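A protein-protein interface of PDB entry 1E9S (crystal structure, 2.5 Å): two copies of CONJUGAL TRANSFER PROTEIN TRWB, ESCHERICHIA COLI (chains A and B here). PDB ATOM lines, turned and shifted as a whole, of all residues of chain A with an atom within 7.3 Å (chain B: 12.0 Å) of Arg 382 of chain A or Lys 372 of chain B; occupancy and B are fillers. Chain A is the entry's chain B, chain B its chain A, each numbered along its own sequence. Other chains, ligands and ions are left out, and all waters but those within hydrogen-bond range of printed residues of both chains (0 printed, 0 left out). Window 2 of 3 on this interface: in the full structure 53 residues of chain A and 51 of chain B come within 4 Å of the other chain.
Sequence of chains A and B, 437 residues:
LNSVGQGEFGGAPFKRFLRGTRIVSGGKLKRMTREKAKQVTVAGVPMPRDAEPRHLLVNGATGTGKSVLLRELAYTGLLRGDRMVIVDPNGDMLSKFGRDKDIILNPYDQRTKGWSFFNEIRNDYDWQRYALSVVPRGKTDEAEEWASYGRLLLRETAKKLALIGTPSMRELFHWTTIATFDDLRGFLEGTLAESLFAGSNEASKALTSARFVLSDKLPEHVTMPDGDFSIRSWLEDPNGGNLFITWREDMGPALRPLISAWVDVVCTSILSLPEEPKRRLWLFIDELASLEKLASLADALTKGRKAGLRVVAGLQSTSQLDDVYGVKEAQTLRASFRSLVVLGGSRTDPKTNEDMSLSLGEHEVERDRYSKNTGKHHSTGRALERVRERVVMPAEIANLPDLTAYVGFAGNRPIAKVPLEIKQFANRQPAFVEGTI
The backbone carbonyl oxygen (O) of Tyr 370 of chain B sits at hydrogen-bond distance from the backbone NH (N) of Leu 384 of chain A (3.5 Å). The backbone NH (N) of Lys 372 of chain B lies within hydrogen-bond range of the backbone carbonyl oxygen (O) of Arg 382 of chain A (3.2 Å). The guanidinium group (NH1) of Arg 369 of chain B lies close to the guanidinium group (NH1) of Arg 369 of chain A (3.1 Å).
The backbone carbonyl oxygen (O) of Ala 383 of chain B is in hydrogen-bond range of the backbone NH (N) of Arg 369 of chain B. NE of Arg 382 of chain A lies within salt-bridge range of OD2 of Asp 368 of chain A (3.1 Å). N of Arg 369 of chain A lies within hydrogen-bond range of O of Ala 383 of chain A (2.7 Å).
O of Arg 382 of chain A touches OG of Ser 371 of chain B, at 3.7 Å. Tyr 370 of chain B touches Ala 383 of chain A. Arg 369 of chain B touches Leu 384 of chain A (CG to O, 3.2 Å).
Arg 382 of chain A touches two residues of chain B. Of the printed residues of chain A, Lys 372 of chain B touches Arg 382 (3.2 Å). No residue of chain B comes within 4 Å of Asp 368 of chain A. No residue of chain B comes within 4 Å of Tyr 370 of chain A. Of chain B, only Arg 369 and Tyr 370 come within 4 Å of Leu 384 of chain A. Printed residues of chain A within 4 Å of Arg 369 of chain B: Arg 369 and Leu 384. Printed residues of chain A within 4 Å of Tyr 370 of chain B: Ala 383 (3.95 Å) and Leu 384 (3.5 Å). Of the printed residues of chain A, Ser 371 of chain B touches Arg 382 (3.7 Å). Printed residues of chain B within 4 Å of Arg 369 of chain A: Arg 369. Lys 15 of chain A touches none of the printed residues of chain B. Asp 368 of chain B touches none of the printed residues of chain A. The nearest residue of chain B that does not touch Arg 382 of chain A is Tyr 370 of chain B (5.2 Å). The nearest residue of chain A that does not touch Lys 372 of chain B is Tyr 370 of chain A (5.0 Å).
Of the 7 printed residues of chain B, 4 touch a printed residue of chain A. Along chain B the printed residues that touch a printed residue of chain A span positions 369 to 372. Among the printed residues, no Asp or Glu carboxylate lies within 4 Å of a Lys or Arg side-chain nitrogen of the other chain.
Arg 369 of chain B touches its own counterpart, Arg 369 of chain A. Ala 383 of chain A touches Tyr 370 of chain B, but with the chains exchanged Tyr 370 of chain A does not touch Ala 383 of chain B (15.2 Å). 5 positions are printed for both chains.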
ATOM      1  N   LYS A  15     -31.553 -28.209 -38.636  1.00  0.00           N
ATOM      2  CA  LYS A  15     -30.940 -29.315 -37.927  1.00  0.00           C
ATOM      3  C   LYS A  15     -31.885 -30.485 -37.697  1.00  0.00           C
ATOM      4  O   LYS A  15     -31.514 -31.635 -37.937  1.00  0.00           O
ATOM      5  CB  LYS A  15     -30.376 -28.838 -36.585  1.00  0.00           C
ATOM      6  CG  LYS A  15     -29.991 -29.978 -35.653  1.00  0.00           C
ATOM      7  CD  LYS A  15     -29.429 -29.489 -34.325  1.00  0.00           C
ATOM      8  CE  LYS A  15     -27.931 -29.203 -34.412  1.00  0.00           C
ATOM      9  NZ  LYS A  15     -27.118 -30.421 -34.713  1.00  0.00           N
ATOM     10  N   ASP A 368     -30.043 -24.005 -36.373  1.00  0.00           N
ATOM     11  CA  ASP A 368     -28.941 -23.353 -35.668  1.00  0.00           C
ATOM     12  C   ASP A 368     -28.754 -21.926 -36.165  1.00  0.00           C
ATOM     13  O   ASP A 368     -28.629 -21.687 -37.367  1.00  0.00           O
ATOM     14  CB  ASP A 368     -27.631 -24.119 -35.873  1.00  0.00           C
ATOM     15  CG  ASP A 368     -27.527 -25.354 -35.007  1.00  0.00           C
ATOM     16  OD1 ASP A 368     -28.470 -25.635 -34.234  1.00  0.00           O
ATOM     17  OD2 ASP A 368     -26.492 -26.048 -35.101  1.00  0.00           O
ATOM     18  N   ARG A 369     -28.740 -20.979 -35.234  1.00  0.00           N
ATOM     19  CA  ARG A 369     -28.534 -19.575 -35.569  1.00  0.00           C
ATOM     20  C   ARG A 369     -27.122 -19.174 -35.144  1.00  0.00           C
ATOM     21  O   ARG A 369     -26.866 -18.973 -33.960  1.00  0.00           O
ATOM     22  CB  ARG A 369     -29.559 -18.698 -34.841  1.00  0.00           C
ATOM     23  CG  ARG A 369     -29.953 -19.208 -33.458  1.00  0.00           C
ATOM     24  CD  ARG A 369     -30.056 -18.088 -32.425  1.00  0.00           C
ATOM     25  NE  ARG A 369     -31.053 -17.074 -32.766  1.00  0.00           N
ATOM     26  CZ  ARG A 369     -31.288 -15.980 -32.045  1.00  0.00           C
ATOM     27  NH1 ARG A 369     -30.597 -15.754 -30.934  1.00  0.00           N
ATOM     28  NH2 ARG A 369     -32.215 -15.109 -32.432  1.00  0.00           N
ATOM     29  N   TYR A 370     -26.204 -19.054 -36.098  1.00  0.00           N
ATOM     30  CA  TYR A 370     -24.832 -18.682 -35.759  1.00  0.00           C
ATOM     31  C   TYR A 370     -24.616 -17.167 -35.750  1.00  0.00           C
ATOM     32  O   TYR A 370     -24.746 -16.495 -36.773  1.00  0.00           O
ATOM     33  CB  TYR A 370     -23.842 -19.347 -36.725  1.00  0.00           C
ATOM     34  CG  TYR A 370     -23.792 -20.866 -36.630  1.00  0.00           C
ATOM     35  CD1 TYR A 370     -24.872 -21.651 -37.039  1.00  0.00           C
ATOM     36  CD2 TYR A 370     -22.654 -21.523 -36.142  1.00  0.00           C
ATOM     37  CE1 TYR A 370     -24.822 -23.051 -36.969  1.00  0.00           C
ATOM     38  CE2 TYR A 370     -22.596 -22.926 -36.065  1.00  0.00           C
ATOM     39  CZ  TYR A 370     -23.684 -23.680 -36.484  1.00  0.00           C
ATOM     40  OH  TYR A 370     -23.638 -25.057 -36.427  1.00  0.00           O
ATOM     41  N   ARG A 382     -23.614 -19.632 -32.141  1.00  0.00           N
ATOM     42  CA  ARG A 382     -24.464 -20.771 -32.477  1.00  0.00           C
ATOM     43  C   ARG A 382     -25.464 -21.115 -31.365  1.00  0.00           C
ATOM     44  O   ARG A 382     -25.068 -21.383 -30.230  1.00  0.00           O
ATOM     45  CB  ARG A 382     -23.599 -21.993 -32.766  1.00  0.00           C
ATOM     46  CG  ARG A 382     -24.398 -23.238 -33.050  1.00  0.00           C
ATOM     47  CD  ARG A 382     -23.608 -24.469 -32.673  1.00  0.00           C
ATOM     48  NE  ARG A 382     -24.383 -25.693 -32.856  1.00  0.00           N
ATOM     49  CZ  ARG A 382     -23.969 -26.900 -32.484  1.00  0.00           C
ATOM     50  NH1 ARG A 382     -22.784 -27.048 -31.900  1.00  0.00           N
ATOM     51  NH2 ARG A 382     -24.733 -27.962 -32.704  1.00  0.00           N
ATOM     52  N   ALA A 383     -26.755 -21.120 -31.709  1.00  0.00           N
ATOM     53  CA  ALA A 383     -27.847 -21.422 -30.771  1.00  0.00           C
ATOM     54  C   ALA A 383     -29.005 -22.111 -31.509  1.00  0.00           C
ATOM     55  O   ALA A 383     -29.121 -21.995 -32.733  1.00  0.00           O
ATOM     56  CB  ALA A 383     -28.343 -20.128 -30.116  1.00  0.00           C
ATOM     57  N   LEU A 384     -29.859 -22.821 -30.770  1.00  0.00           N
ATOM     58  CA  LEU A 384     -31.003 -23.510 -31.376  1.00  0.00           C
ATOM     59  C   LEU A 384     -32.299 -22.701 -31.284  1.00  0.00           C
ATOM     60  O   LEU A 384     -32.614 -22.127 -30.241  1.00  0.00           O
ATOM     61  CB  LEU A 384     -31.211 -24.885 -30.736  1.00  0.00           C
ATOM     62  CG  LEU A 384     -30.652 -26.084 -31.509  1.00  0.00           C
ATOM     63  CD1 LEU A 384     -30.940 -27.365 -30.745  1.00  0.00           C
ATOM     64  CD2 LEU A 384     -31.280 -26.149 -32.886  1.00  0.00           C
ATOM     65  N   ASP B 368     -36.244 -24.886 -22.615  1.00  0.00           N
ATOM     66  CA  ASP B 368     -34.862 -24.439 -22.525  1.00  0.00           C
ATOM     67  C   ASP B 368     -34.286 -24.201 -23.910  1.00  0.00           C
ATOM     68  O   ASP B 368     -34.306 -25.091 -24.760  1.00  0.00           O
ATOM     69  CB  ASP B 368     -34.019 -25.479 -21.790  1.00  0.00           C
ATOM     70  CG  ASP B 368     -34.213 -25.422 -20.282  1.00  0.00           C
ATOM     71  OD1 ASP B 368     -34.597 -24.350 -19.758  1.00  0.00           O
ATOM     72  OD2 ASP B 368     -33.966 -26.448 -19.616  1.00  0.00           O
ATOM     73  N   ARG B 369     -33.786 -22.992 -24.140  1.00  0.00           N
ATOM     74  CA  ARG B 369     -33.189 -22.647 -25.426  1.00  0.00           C
ATOM     75  C   ARG B 369     -31.673 -22.710 -25.227  1.00  0.00           C
ATOM     76  O   ARG B 369     -31.040 -21.721 -24.851  1.00  0.00           O
ATOM     77  CB  ARG B 369     -33.614 -21.229 -25.857  1.00  0.00           C
ATOM     78  CG  ARG B 369     -33.399 -20.913 -27.349  1.00  0.00           C
ATOM     79  CD  ARG B 369     -33.128 -19.423 -27.633  1.00  0.00           C
ATOM     80  NE  ARG B 369     -31.811 -18.996 -27.151  1.00  0.00           N
ATOM     81  CZ  ARG B 369     -31.204 -17.861 -27.495  1.00  0.00           C
ATOM     82  NH1 ARG B 369     -31.780 -17.022 -28.346  1.00  0.00           N
ATOM     83  NH2 ARG B 369     -30.008 -17.570 -26.993  1.00  0.00           N
ATOM     84  N   TYR B 370     -31.098 -23.885 -25.458  1.00  0.00           N
ATOM     85  CA  TYR B 370     -29.663 -24.086 -25.291  1.00  0.00           C
ATOM     86  C   TYR B 370     -28.768 -23.288 -26.239  1.00  0.00           C
ATOM     87  O   TYR B 370     -29.131 -23.018 -27.392  1.00  0.00           O
ATOM     88  CB  TYR B 370     -29.339 -25.575 -25.406  1.00  0.00           C
ATOM     89  CG  TYR B 370     -29.404 -26.294 -24.077  1.00  0.00           C
ATOM     90  CD1 TYR B 370     -30.558 -26.262 -23.292  1.00  0.00           C
ATOM     91  CD2 TYR B 370     -28.299 -26.986 -23.592  1.00  0.00           C
ATOM     92  CE1 TYR B 370     -30.608 -26.899 -22.057  1.00  0.00           C
ATOM     93  CE2 TYR B 370     -28.338 -27.627 -22.361  1.00  0.00           C
ATOM     94  CZ  TYR B 370     -29.494 -27.579 -21.598  1.00  0.00           C
ATOM     95  OH  TYR B 370     -29.527 -28.212 -20.376  1.00  0.00           O
ATOM     96  N   SER B 371     -27.585 -22.931 -25.736  1.00  0.00           N
ATOM     97  CA  SER B 371     -26.601 -22.167 -26.500  1.00  0.00           C
ATOM     98  C   SER B 371     -25.165 -22.684 -26.283  1.00  0.00           C
ATOM     99  O   SER B 371     -24.864 -23.329 -25.274  1.00  0.00           O
ATOM    100  CB  SER B 371     -26.694 -20.684 -26.124  1.00  0.00           C
ATOM    101  OG  SER B 371     -25.875 -19.890 -26.960  1.00  0.00           O
ATOM    102  N   LYS B 372     -24.289 -22.403 -27.250  1.00  0.00           N
ATOM    103  CA  LYS B 372     -22.891 -22.834 -27.208  1.00  0.00           C
ATOM    104  C   LYS B 372     -21.960 -21.634 -27.062  1.00  0.00           C
ATOM    105  O   LYS B 372     -21.513 -21.312 -25.959  1.00  0.00           O
ATOM    106  CB  LYS B 372     -22.540 -23.608 -28.488  1.00  0.00           C
ATOM    107  CG  LYS B 372     -21.187 -24.317 -28.453  1.00  0.00           C
ATOM    108  CD  LYS B 372     -20.917 -25.137 -29.721  1.00  0.00           C
ATOM    109  CE  LYS B 372     -20.659 -24.251 -30.931  1.00  0.00           C
ATOM    110  NZ  LYS B 372     -20.341 -25.047 -32.147  1.00  0.00           N
ATOM    111  N   ARG B 382     -27.849 -21.560 -21.917  1.00  0.00           N
ATOM    112  CA  ARG B 382     -29.102 -22.079 -21.370  1.00  0.00           C
ATOM    113  C   ARG B 382     -30.059 -20.984 -20.892  1.00  0.00           C
ATOM    114  O   ARG B 382     -29.749 -20.235 -19.965  1.00  0.00           O
ATOM    115  CB  ARG B 382     -28.804 -23.039 -20.218  1.00  0.00           C
ATOM    116  CG  ARG B 382     -29.988 -23.321 -19.300  1.00  0.00           C
ATOM    117  CD  ARG B 382     -29.689 -24.533 -18.436  1.00  0.00           C
ATOM    118  NE  ARG B 382     -30.624 -24.710 -17.327  1.00  0.00           N
ATOM    119  CZ  ARG B 382     -30.753 -25.847 -16.646  1.00  0.00           C
ATOM    120  NH1 ARG B 382     -30.009 -26.898 -16.972  1.00  0.00           N
ATOM    121  NH2 ARG B 382     -31.616 -25.938 -15.638  1.00  0.00           N
ATOM    122  N   ALA B 383     -31.236 -20.915 -21.511  1.00  0.00           N
ATOM    123  CA  ALA B 383     -32.227 -19.903 -21.160  1.00  0.00           C
ATOM    124  C   ALA B 383     -33.654 -20.443 -21.227  1.00  0.00           C
ATOM    125  O   ALA B 383     -33.993 -21.230 -22.112  1.00  0.00           O
ATOM    126  CB  ALA B 383     -32.081 -18.701 -22.088  1.00  0.00           C
